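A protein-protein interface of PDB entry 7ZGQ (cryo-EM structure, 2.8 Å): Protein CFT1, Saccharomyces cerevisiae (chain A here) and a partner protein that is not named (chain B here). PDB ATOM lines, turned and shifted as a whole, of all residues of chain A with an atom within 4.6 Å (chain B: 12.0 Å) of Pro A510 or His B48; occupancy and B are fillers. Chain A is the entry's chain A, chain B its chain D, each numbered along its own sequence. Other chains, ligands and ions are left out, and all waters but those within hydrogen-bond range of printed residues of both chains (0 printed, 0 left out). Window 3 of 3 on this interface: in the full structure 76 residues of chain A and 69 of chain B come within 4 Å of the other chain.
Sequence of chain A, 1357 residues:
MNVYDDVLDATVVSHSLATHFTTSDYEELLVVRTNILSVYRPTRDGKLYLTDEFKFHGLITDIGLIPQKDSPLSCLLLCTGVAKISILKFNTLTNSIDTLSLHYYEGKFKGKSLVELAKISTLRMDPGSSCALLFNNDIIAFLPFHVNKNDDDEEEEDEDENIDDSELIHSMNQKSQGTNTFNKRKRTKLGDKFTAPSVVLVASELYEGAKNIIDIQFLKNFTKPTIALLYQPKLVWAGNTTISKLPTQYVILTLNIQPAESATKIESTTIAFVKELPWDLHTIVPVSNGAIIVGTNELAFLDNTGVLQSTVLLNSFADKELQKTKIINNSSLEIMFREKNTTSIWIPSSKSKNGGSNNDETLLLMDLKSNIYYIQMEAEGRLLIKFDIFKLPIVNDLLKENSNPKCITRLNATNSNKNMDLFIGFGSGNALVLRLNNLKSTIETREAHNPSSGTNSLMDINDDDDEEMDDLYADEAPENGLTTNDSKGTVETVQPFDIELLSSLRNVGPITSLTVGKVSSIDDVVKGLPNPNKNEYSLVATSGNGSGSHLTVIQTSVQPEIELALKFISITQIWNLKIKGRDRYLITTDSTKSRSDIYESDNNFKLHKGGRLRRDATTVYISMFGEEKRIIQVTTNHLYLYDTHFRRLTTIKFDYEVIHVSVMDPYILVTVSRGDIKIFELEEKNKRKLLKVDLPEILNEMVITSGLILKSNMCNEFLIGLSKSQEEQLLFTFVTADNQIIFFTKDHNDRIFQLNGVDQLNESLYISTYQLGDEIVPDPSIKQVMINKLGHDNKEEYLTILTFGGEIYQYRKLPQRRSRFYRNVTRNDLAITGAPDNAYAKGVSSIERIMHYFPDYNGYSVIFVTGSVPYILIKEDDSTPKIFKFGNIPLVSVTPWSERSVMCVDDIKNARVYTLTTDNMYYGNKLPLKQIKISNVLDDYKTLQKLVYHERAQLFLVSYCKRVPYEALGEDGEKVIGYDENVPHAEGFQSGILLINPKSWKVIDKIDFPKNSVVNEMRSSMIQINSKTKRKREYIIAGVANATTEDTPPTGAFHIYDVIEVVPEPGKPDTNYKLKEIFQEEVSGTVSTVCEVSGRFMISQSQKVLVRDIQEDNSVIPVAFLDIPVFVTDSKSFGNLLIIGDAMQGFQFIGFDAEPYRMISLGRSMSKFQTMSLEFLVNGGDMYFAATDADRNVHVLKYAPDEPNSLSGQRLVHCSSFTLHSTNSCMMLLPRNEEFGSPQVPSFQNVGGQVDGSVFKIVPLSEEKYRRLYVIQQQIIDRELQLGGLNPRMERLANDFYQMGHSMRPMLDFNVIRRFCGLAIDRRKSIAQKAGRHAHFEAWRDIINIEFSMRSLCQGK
The side-chain amide oxygen (OE1) of Gln A945 sits at hydrogen-bond distance from a ring nitrogen (NE2) of His B48 (2.7 Å).
The backbone carbonyl oxygen (O) of His B48 sits at hydrogen-bond distance from the side-chain amide nitrogen (ND2) of Asn A545, at 2.6 Å.
The side-chain hydroxyl of Thr A542 is in hydrogen-bond range of the side-chain hydroxyl of Thr A512 (2.7 Å).
N of Gly A544 is in hydrogen-bond range of O of Pro A510 (3.5 Å).
The backbone NH of Asn A545 is in hydrogen-bond range of the side-chain hydroxyl of Ser A428 (2.8 Å).
The backbone carbonyl oxygen of Asn B45 lies within hydrogen-bond range of the backbone NH of Leu B50 (2.9 Å).
CG of Pro A510 touches O of His B48 (3.3 Å).
ND1 of His B48 touches CG2 of Thr A512, at 3.6 Å.
Leu B50 touches Asn A545.
CG2 of Thr A943 touches OH of Tyr B44, at 3.3 Å.
Thr A943 touches His B48.
OE1 of Gln A945 touches CE1 of Tyr B44 (3.2 Å).
Val A1251 touches Arg B46 (CG2 to O, 3.8 Å).
Val A1251 touches Arg B47 (CG2 to O, 3.3 Å).
Val A1251 touches Gly B49 (CG2 to N, 3.6 Å).
Pro A510 touches just one residue of chain B: His B48.
His B48 touches just these residues of chain A: Pro A510, Thr A512, Asn A545, Thr A943 and Gln A945.
Gly A427 touches none of the printed residues of chain B.
No residue of chain B comes within 4 Å of Ser A428.
Val A508 touches none of the printed residues of chain B.
No residue of chain B comes within 4 Å of Ile A511.
Of chain B, only His B48 comes within 4 Å of Thr A512.
Ser A543 touches none of the printed residues of chain B.
No residue of chain B comes within 4 Å of Gly A544.
Val A1251 touches just these residues of chain B: Arg B46 (3.8 Å), Arg B47 (3.3 Å) and Gly B49 (3.6 Å).
Printed residues of chain A within 4 Å of Gly B49: Val A1251 (3.6 Å).
Printed residues of chain A within 4 Å of Arg B46: Val A1251.
Printed residues of chain A that touch a printed residue of chain B: Pro A510, Thr A512, Asn A545, Thr A943, Gln A945 and Val A1251.
Of the 16 printed residues of chain B, 6 touch a printed residue of chain A.
Printed residues of chain B that touch a printed residue of chain A: Tyr B44, Arg B46, Arg B47, His B48, Gly B49 and Leu B50.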
ATOM      1  N   GLY A 427       6.449  10.091  12.696  1.00  0.00           N
ATOM      2  CA  GLY A 427       5.744   9.981  11.435  1.00  0.00           C
ATOM      3  C   GLY A 427       6.170  11.002  10.401  1.00  0.00           C
ATOM      4  O   GLY A 427       6.189  10.705   9.203  1.00  0.00           O
ATOM      5  N   SER A 428       6.511  12.212  10.845  1.00  0.00           N
ATOM      6  CA  SER A 428       6.907  13.285   9.942  1.00  0.00           C
ATOM      7  C   SER A 428       8.409  13.537   9.981  1.00  0.00           C
ATOM      8  O   SER A 428       9.076  13.463   8.946  1.00  0.00           O
ATOM      9  CB  SER A 428       6.140  14.569  10.280  1.00  0.00           C
ATOM     10  OG  SER A 428       6.661  15.675   9.564  1.00  0.00           O
ATOM     11  N   VAL A 508      12.048  10.862   5.390  1.00  0.00           N
ATOM     12  CA  VAL A 508      11.569  11.837   4.420  1.00  0.00           C
ATOM     13  C   VAL A 508      10.081  12.053   4.654  1.00  0.00           C
ATOM     14  O   VAL A 508       9.370  12.561   3.781  1.00  0.00           O
ATOM     15  CB  VAL A 508      11.857  11.390   2.975  1.00  0.00           C
ATOM     16  CG1 VAL A 508      13.340  11.113   2.791  1.00  0.00           C
ATOM     17  CG2 VAL A 508      11.040  10.164   2.618  1.00  0.00           C
ATOM     18  N   GLY A 509       9.603  11.653   5.831  1.00  0.00           N
ATOM     19  CA  GLY A 509       8.230  11.865   6.224  1.00  0.00           C
ATOM     20  C   GLY A 509       7.265  11.253   5.236  1.00  0.00           C
ATOM     21  O   GLY A 509       7.589  10.295   4.532  1.00  0.00           O
ATOM     22  N   PRO A 510       6.051  11.797   5.162  1.00  0.00           N
ATOM     23  CA  PRO A 510       5.145  11.419   4.073  1.00  0.00           C
ATOM     24  C   PRO A 510       5.459  12.233   2.825  1.00  0.00           C
ATOM     25  O   PRO A 510       5.500  13.464   2.865  1.00  0.00           O
ATOM     26  CB  PRO A 510       3.758  11.752   4.630  1.00  0.00           C
ATOM     27  CG  PRO A 510       4.006  12.847   5.602  1.00  0.00           C
ATOM     28  CD  PRO A 510       5.396  12.664   6.156  1.00  0.00           C
ATOM     29  N   ILE A 511       5.693  11.536   1.716  1.00  0.00           N
ATOM     30  CA  ILE A 511       5.943  12.197   0.439  1.00  0.00           C
ATOM     31  C   ILE A 511       4.519  12.610   0.081  1.00  0.00           C
ATOM     32  O   ILE A 511       3.613  11.778   0.016  1.00  0.00           O
ATOM     33  CB  ILE A 511       6.687  11.290  -0.541  1.00  0.00           C
ATOM     34  CG1 ILE A 511       8.151  11.163  -0.117  1.00  0.00           C
ATOM     35  CG2 ILE A 511       6.614  11.848  -1.950  1.00  0.00           C
ATOM     36  CD1 ILE A 511       8.705   9.773  -0.253  1.00  0.00           C
ATOM     37  N   THR A 512       4.314  13.909  -0.133  1.00  0.00           N
ATOM     38  CA  THR A 512       2.983  14.458  -0.334  1.00  0.00           C
ATOM     39  C   THR A 512       2.868  14.939  -1.772  1.00  0.00           C
ATOM     40  O   THR A 512       1.746  15.068  -2.275  1.00  0.00           O
ATOM     41  CB  THR A 512       2.622  15.612   0.609  1.00  0.00           C
ATOM     42  OG1 THR A 512       3.609  16.646   0.500  1.00  0.00           O
ATOM     43  CG2 THR A 512       2.572  15.124   2.046  1.00  0.00           C
ATOM     44  N   THR A 542       8.029  16.860  -1.891  1.00  0.00           N
ATOM     45  CA  THR A 542       7.779  17.508  -0.613  1.00  0.00           C
ATOM     46  C   THR A 542       7.722  16.454   0.482  1.00  0.00           C
ATOM     47  O   THR A 542       7.158  15.372   0.295  1.00  0.00           O
ATOM     48  CB  THR A 542       6.473  18.301  -0.648  1.00  0.00           C
ATOM     49  OG1 THR A 542       5.446  17.505  -1.248  1.00  0.00           O
ATOM     50  CG2 THR A 542       6.650  19.580  -1.447  1.00  0.00           C
ATOM     51  N   SER A 543       8.311  16.772   1.629  1.00  0.00           N
ATOM     52  CA  SER A 543       8.478  15.810   2.704  1.00  0.00           C
ATOM     53  C   SER A 543       7.984  16.404   4.014  1.00  0.00           C
ATOM     54  O   SER A 543       8.089  17.608   4.250  1.00  0.00           O
ATOM     55  CB  SER A 543       9.945  15.390   2.841  1.00  0.00           C
ATOM     56  OG  SER A 543      10.276  14.379   1.904  1.00  0.00           O
ATOM     57  N   GLY A 544       7.429  15.541   4.859  1.00  0.00           N
ATOM     58  CA  GLY A 544       7.050  15.921   6.203  1.00  0.00           C
ATOM     59  C   GLY A 544       5.749  16.699   6.265  1.00  0.00           C
ATOM     60  O   GLY A 544       5.170  17.110   5.258  1.00  0.00           O
ATOM     61  N   ASN A 545       5.284  16.905   7.499  1.00  0.00           N
ATOM     62  CA  ASN A 545       4.087  17.703   7.786  1.00  0.00           C
ATOM     63  C   ASN A 545       4.467  18.707   8.869  1.00  0.00           C
ATOM     64  O   ASN A 545       4.990  18.332   9.922  1.00  0.00           O
ATOM     65  CB  ASN A 545       2.914  16.836   8.224  1.00  0.00           C
ATOM     66  CG  ASN A 545       2.674  15.667   7.304  1.00  0.00           C
ATOM     67  OD1 ASN A 545       2.696  15.808   6.082  1.00  0.00           O
ATOM     68  ND2 ASN A 545       2.431  14.501   7.886  1.00  0.00           N
ATOM     69  N   THR A 943       4.006  23.023   6.438  1.00  0.00           N
ATOM     70  CA  THR A 943       3.917  21.927   5.482  1.00  0.00           C
ATOM     71  C   THR A 943       3.863  22.442   4.051  1.00  0.00           C
ATOM     72  O   THR A 943       3.148  23.399   3.744  1.00  0.00           O
ATOM     73  CB  THR A 943       2.693  21.059   5.787  1.00  0.00           C
ATOM     74  OG1 THR A 943       2.413  20.208   4.668  1.00  0.00           O
ATOM     75  CG2 THR A 943       1.488  21.919   6.098  1.00  0.00           C
ATOM     76  N   GLN A 945       3.427  21.430  -0.150  1.00  0.00           N
ATOM     77  CA  GLN A 945       2.721  20.466  -0.976  1.00  0.00           C
ATOM     78  C   GLN A 945       2.528  21.031  -2.374  1.00  0.00           C
ATOM     79  O   GLN A 945       2.686  22.232  -2.608  1.00  0.00           O
ATOM     80  CB  GLN A 945       1.367  20.100  -0.361  1.00  0.00           C
ATOM     81  CG  GLN A 945       0.532  21.305   0.029  1.00  0.00           C
ATOM     82  CD  GLN A 945      -0.627  20.940   0.928  1.00  0.00           C
ATOM     83  OE1 GLN A 945      -0.680  19.839   1.474  1.00  0.00           O
ATOM     84  NE2 GLN A 945      -1.565  21.865   1.089  1.00  0.00           N
ATOM     85  N   GLN A1250       4.535   7.852  -1.007  1.00  0.00           N
ATOM     86  CA  GLN A1250       3.792   7.151   0.027  1.00  0.00           C
ATOM     87  C   GLN A1250       3.887   7.886   1.356  1.00  0.00           C
ATOM     88  O   GLN A1250       4.795   8.689   1.589  1.00  0.00           O
ATOM     89  CB  GLN A1250       4.297   5.715   0.193  1.00  0.00           C
ATOM     90  CG  GLN A1250       4.258   4.894  -1.078  1.00  0.00           C
ATOM     91  CD  GLN A1250       3.109   3.913  -1.094  1.00  0.00           C
ATOM     92  OE1 GLN A1250       1.977   4.274  -1.410  1.00  0.00           O
ATOM     93  NE2 GLN A1250       3.392   2.663  -0.753  1.00  0.00           N
ATOM     94  N   VAL A1251       2.923   7.594   2.229  1.00  0.00           N
ATOM     95  CA  VAL A1251       2.888   8.213   3.550  1.00  0.00           C
ATOM     96  C   VAL A1251       4.063   7.739   4.398  1.00  0.00           C
ATOM     97  O   VAL A1251       4.633   8.509   5.178  1.00  0.00           O
ATOM     98  CB  VAL A1251       1.533   7.929   4.225  1.00  0.00           C
ATOM     99  CG1 VAL A1251       1.661   7.939   5.741  1.00  0.00           C
ATOM    100  CG2 VAL A1251       0.497   8.943   3.772  1.00  0.00           C
ATOM    101  N   TYR B  39     -14.722  16.439   2.799  1.00  0.00           N
ATOM    102  CA  TYR B  39     -13.893  15.530   2.013  1.00  0.00           C
ATOM    103  C   TYR B  39     -12.520  16.127   1.738  1.00  0.00           C
ATOM    104  O   TYR B  39     -11.519  15.402   1.706  1.00  0.00           O
ATOM    105  CB  TYR B  39     -14.600  15.167   0.710  1.00  0.00           C
ATOM    106  CG  TYR B  39     -15.273  13.823   0.779  1.00  0.00           C
ATOM    107  CD1 TYR B  39     -14.554  12.687   1.117  1.00  0.00           C
ATOM    108  CD2 TYR B  39     -16.629  13.689   0.533  1.00  0.00           C
ATOM    109  CE1 TYR B  39     -15.163  11.456   1.197  1.00  0.00           C
ATOM    110  CE2 TYR B  39     -17.249  12.461   0.607  1.00  0.00           C
ATOM    111  CZ  TYR B  39     -16.509  11.348   0.939  1.00  0.00           C
ATOM    112  OH  TYR B  39     -17.117  10.121   1.017  1.00  0.00           O
ATOM    113  N   ILE B  40     -12.450  17.445   1.542  1.00  0.00           N
ATOM    114  CA  ILE B  40     -11.156  18.110   1.414  1.00  0.00           C
ATOM    115  C   ILE B  40     -10.325  17.876   2.668  1.00  0.00           C
ATOM    116  O   ILE B  40      -9.146  17.504   2.599  1.00  0.00           O
ATOM    117  CB  ILE B  40     -11.349  19.612   1.139  1.00  0.00           C
ATOM    118  CG1 ILE B  40     -11.949  19.837  -0.250  1.00  0.00           C
ATOM    119  CG2 ILE B  40     -10.035  20.361   1.302  1.00  0.00           C
ATOM    120  CD1 ILE B  40     -10.926  19.863  -1.364  1.00  0.00           C
ATOM    121  N   ASN B  41     -10.941  18.071   3.836  1.00  0.00           N
ATOM    122  CA  ASN B  41     -10.240  17.842   5.097  1.00  0.00           C
ATOM    123  C   ASN B  41      -9.826  16.381   5.245  1.00  0.00           C
ATOM    124  O   ASN B  41      -8.698  16.084   5.661  1.00  0.00           O
ATOM    125  CB  ASN B  41     -11.125  18.269   6.268  1.00  0.00           C
ATOM    126  CG  ASN B  41     -10.328  18.588   7.515  1.00  0.00           C
ATOM    127  OD1 ASN B  41      -9.106  18.713   7.472  1.00  0.00           O
ATOM    128  ND2 ASN B  41     -11.021  18.719   8.640  1.00  0.00           N
ATOM    129  N   LEU B  42     -10.726  15.457   4.902  1.00  0.00           N
ATOM    130  CA  LEU B  42     -10.429  14.037   5.044  1.00  0.00           C
ATOM    131  C   LEU B  42      -9.257  13.627   4.171  1.00  0.00           C
ATOM    132  O   LEU B  42      -8.362  12.907   4.623  1.00  0.00           O
ATOM    133  CB  LEU B  42     -11.658  13.200   4.697  1.00  0.00           C
ATOM    134  CG  LEU B  42     -11.366  11.720   4.435  1.00  0.00           C
ATOM    135  CD1 LEU B  42     -11.104  10.990   5.741  1.00  0.00           C
ATOM    136  CD2 LEU B  42     -12.498  11.061   3.668  1.00  0.00           C
ATOM    137  N   TYR B  43      -9.235  14.080   2.919  1.00  0.00           N
ATOM    138  CA  TYR B  43      -8.154  13.680   2.033  1.00  0.00           C
ATOM    139  C   TYR B  43      -6.854  14.406   2.348  1.00  0.00           C
ATOM    140  O   TYR B  43      -5.776  13.856   2.104  1.00  0.00           O
ATOM    141  CB  TYR B  43      -8.565  13.885   0.577  1.00  0.00           C
ATOM    142  CG  TYR B  43      -9.226  12.654   0.009  1.00  0.00           C
ATOM    143  CD1 TYR B  43     -10.586  12.437   0.171  1.00  0.00           C
ATOM    144  CD2 TYR B  43      -8.484  11.689  -0.651  1.00  0.00           C
ATOM    145  CE1 TYR B  43     -11.191  11.305  -0.330  1.00  0.00           C
ATOM    146  CE2 TYR B  43      -9.079  10.555  -1.155  1.00  0.00           C
ATOM    147  CZ  TYR B  43     -10.432  10.366  -0.993  1.00  0.00           C
ATOM    148  OH  TYR B  43     -11.029   9.236  -1.496  1.00  0.00           O
ATOM    149  N   TYR B  44      -6.921  15.618   2.903  1.00  0.00           N
ATOM    150  CA  TYR B  44      -5.704  16.248   3.403  1.00  0.00           C
ATOM    151  C   TYR B  44      -5.110  15.443   4.553  1.00  0.00           C
ATOM    152  O   TYR B  44      -3.896  15.224   4.611  1.00  0.00           O
ATOM    153  CB  TYR B  44      -5.985  17.683   3.842  1.00  0.00           C
ATOM    154  CG  TYR B  44      -4.747  18.408   4.316  1.00  0.00           C
ATOM    155  CD1 TYR B  44      -3.926  19.077   3.420  1.00  0.00           C
ATOM    156  CD2 TYR B  44      -4.394  18.416   5.660  1.00  0.00           C
ATOM    157  CE1 TYR B  44      -2.793  19.736   3.847  1.00  0.00           C
ATOM    158  CE2 TYR B  44      -3.262  19.070   6.096  1.00  0.00           C
ATOM    159  CZ  TYR B  44      -2.466  19.730   5.185  1.00  0.00           C
ATOM    160  OH  TYR B  44      -1.337  20.385   5.616  1.00  0.00           O
ATOM    161  N   ASN B  45      -5.957  14.999   5.485  1.00  0.00           N
ATOM    162  CA  ASN B  45      -5.469  14.176   6.588  1.00  0.00           C
ATOM    163  C   ASN B  45      -4.948  12.835   6.089  1.00  0.00           C
ATOM    164  O   ASN B  45      -3.946  12.318   6.597  1.00  0.00           O
ATOM    165  CB  ASN B  45      -6.577  13.968   7.619  1.00  0.00           C
ATOM    166  CG  ASN B  45      -6.846  15.207   8.441  1.00  0.00           C
ATOM    167  OD1 ASN B  45      -6.245  16.258   8.217  1.00  0.00           O
ATOM    168  ND2 ASN B  45      -7.753  15.093   9.403  1.00  0.00           N
ATOM    169  N   ARG B  46      -5.621  12.255   5.095  1.00  0.00           N
ATOM    170  CA  ARG B  46      -5.257  10.931   4.605  1.00  0.00           C
ATOM    171  C   ARG B  46      -3.947  10.962   3.829  1.00  0.00           C
ATOM    172  O   ARG B  46      -3.114  10.060   3.969  1.00  0.00           O
ATOM    173  CB  ARG B  46      -6.386  10.388   3.732  1.00  0.00           C
ATOM    174  CG  ARG B  46      -6.750   8.944   3.986  1.00  0.00           C
ATOM    175  CD  ARG B  46      -7.907   8.528   3.094  1.00  0.00           C
ATOM    176  NE  ARG B  46      -9.134   8.288   3.842  1.00  0.00           N
ATOM    177  CZ  ARG B  46     -10.329   8.146   3.287  1.00  0.00           C
ATOM    178  NH1 ARG B  46     -10.500   8.241   1.979  1.00  0.00           N
ATOM    179  NH2 ARG B  46     -11.381   7.902   4.064  1.00  0.00           N
ATOM    180  N   ARG B  47      -3.746  11.991   3.002  1.00  0.00           N
ATOM    181  CA  ARG B  47      -2.566  12.043   2.147  1.00  0.00           C
ATOM    182  C   ARG B  47      -1.303  12.387   2.922  1.00  0.00           C
ATOM    183  O   ARG B  47      -0.214  11.942   2.548  1.00  0.00           O
ATOM    184  CB  ARG B  47      -2.784  13.052   1.020  1.00  0.00           C
ATOM    185  CG  ARG B  47      -3.379  12.441  -0.231  1.00  0.00           C
ATOM    186  CD  ARG B  47      -3.680  13.489  -1.282  1.00  0.00           C
ATOM    187  NE  ARG B  47      -4.488  12.940  -2.363  1.00  0.00           N
ATOM    188  CZ  ARG B  47      -5.704  13.363  -2.678  1.00  0.00           C
ATOM    189  NH1 ARG B  47      -6.280  14.358  -2.025  1.00  0.00           N
ATOM    190  NH2 ARG B  47      -6.358  12.774  -3.673  1.00  0.00           N
ATOM    191  N   HIS B  48      -1.421  13.170   3.989  1.00  0.00           N
ATOM    192  CA  HIS B  48      -0.276  13.535   4.811  1.00  0.00           C
ATOM    193  C   HIS B  48      -0.022  12.549   5.940  1.00  0.00           C
ATOM    194  O   HIS B  48       0.894  12.767   6.739  1.00  0.00           O
ATOM    195  CB  HIS B  48      -0.468  14.941   5.388  1.00  0.00           C
ATOM    196  CG  HIS B  48      -0.266  16.037   4.388  1.00  0.00           C
ATOM    197  ND1 HIS B  48       0.750  16.960   4.493  1.00  0.00           N
ATOM    198  CD2 HIS B  48      -0.948  16.351   3.262  1.00  0.00           C
ATOM    199  CE1 HIS B  48       0.686  17.799   3.474  1.00  0.00           C
ATOM    200  NE2 HIS B  48      -0.335  17.452   2.713  1.00  0.00           N
ATOM    201  N   GLY B  49      -0.805  11.477   6.030  1.00  0.00           N
ATOM    202  CA  GLY B  49      -0.628  10.510   7.092  1.00  0.00           C
ATOM    203  C   GLY B  49      -1.129  10.954   8.444  1.00  0.00           C
ATOM    204  O   GLY B  49      -0.880  10.264   9.437  1.00  0.00           O
ATOM    205  N   LEU B  50      -1.820  12.086   8.516  1.00  0.00           N
ATOM    206  CA  LEU B  50      -2.332  12.566   9.785  1.00  0.00           C
ATOM    207  C   LEU B  50      -3.536  11.733  10.220  1.00  0.00           C
ATOM    208  O   LEU B  50      -4.331  11.290   9.387  1.00  0.00           O
ATOM    209  CB  LEU B  50      -2.725  14.036   9.679  1.00  0.00           C
ATOM    210  CG  LEU B  50      -1.641  14.967   9.137  1.00  0.00           C
ATOM    211  CD1 LEU B  50      -2.245  16.263   8.629  1.00  0.00           C
ATOM    212  CD2 LEU B  50      -0.596  15.239  10.203  1.00  0.00           C
ATOM    213  N   PRO B  51      -3.691  11.501  11.519  1.00  0.00           N
ATOM    214  CA  PRO B  51      -4.835  10.727  12.006  1.00  0.00           C
ATOM    215  C   PRO B  51      -6.111  11.559  11.993  1.00  0.00           C
ATOM    216  O   PRO B  51      -6.095  12.781  11.847  1.00  0.00           O
ATOM    217  CB  PRO B  51      -4.427  10.359  13.434  1.00  0.00           C
ATOM    218  CG  PRO B  51      -3.520  11.462  13.850  1.00  0.00           C
ATOM    219  CD  PRO B  51      -2.798  11.923  12.613  1.00  0.00           C
ATOM    220  N   ASN B  52      -7.232  10.862  12.147  1.00  0.00           N
ATOM    221  CA  ASN B  52      -8.535  11.513  12.259  1.00  0.00           C
ATOM    222  C   ASN B  52      -8.714  11.953  13.706  1.00  0.00           C
ATOM    223  O   ASN B  52      -9.001  11.139  14.586  1.00  0.00           O
ATOM    224  CB  ASN B  52      -9.649  10.574  11.813  1.00  0.00           C
ATOM    225  CG  ASN B  52      -9.933  10.675  10.331  1.00  0.00           C
ATOM    226  OD1 ASN B  52      -9.502  11.617   9.668  1.00  0.00           O
ATOM    227  ND2 ASN B  52     -10.661   9.700   9.799  1.00  0.00           N
ATOM    228  N   LEU B  53      -8.535  13.247  13.951  1.00  0.00           N
ATOM    229  CA  LEU B  53      -8.572  13.771  15.309  1.00  0.00           C
ATOM    230  C   LEU B  53      -9.963  13.621  15.913  1.00  0.00           C
ATOM    231  O   LEU B  53     -10.976  13.825  15.240  1.00  0.00           O
ATOM    232  CB  LEU B  53      -8.147  15.237  15.317  1.00  0.00           C
ATOM    233  CG  LEU B  53      -6.724  15.502  14.825  1.00  0.00           C
ATOM    234  CD1 LEU B  53      -6.362  16.969  14.975  1.00  0.00           C
ATOM    235  CD2 LEU B  53      -5.736  14.625  15.569  1.00  0.00           C
ATOM    236  N   MET B  66     -15.530  14.191  10.030  1.00  0.00           N
ATOM    237  CA  MET B  66     -15.228  13.617   8.735  1.00  0.00           C
ATOM    238  C   MET B  66     -16.515  13.223   8.016  1.00  0.00           C
ATOM    239  O   MET B  66     -17.571  13.092   8.640  1.00  0.00           O
ATOM    240  CB  MET B  66     -14.316  12.404   8.899  1.00  0.00           C
ATOM    241  CG  MET B  66     -12.852  12.763   9.049  1.00  0.00           C
ATOM    242  SD  MET B  66     -12.401  14.195   8.053  1.00  0.00           S
ATOM    243  CE  MET B  66     -11.821  15.323   9.313  1.00  0.00           C
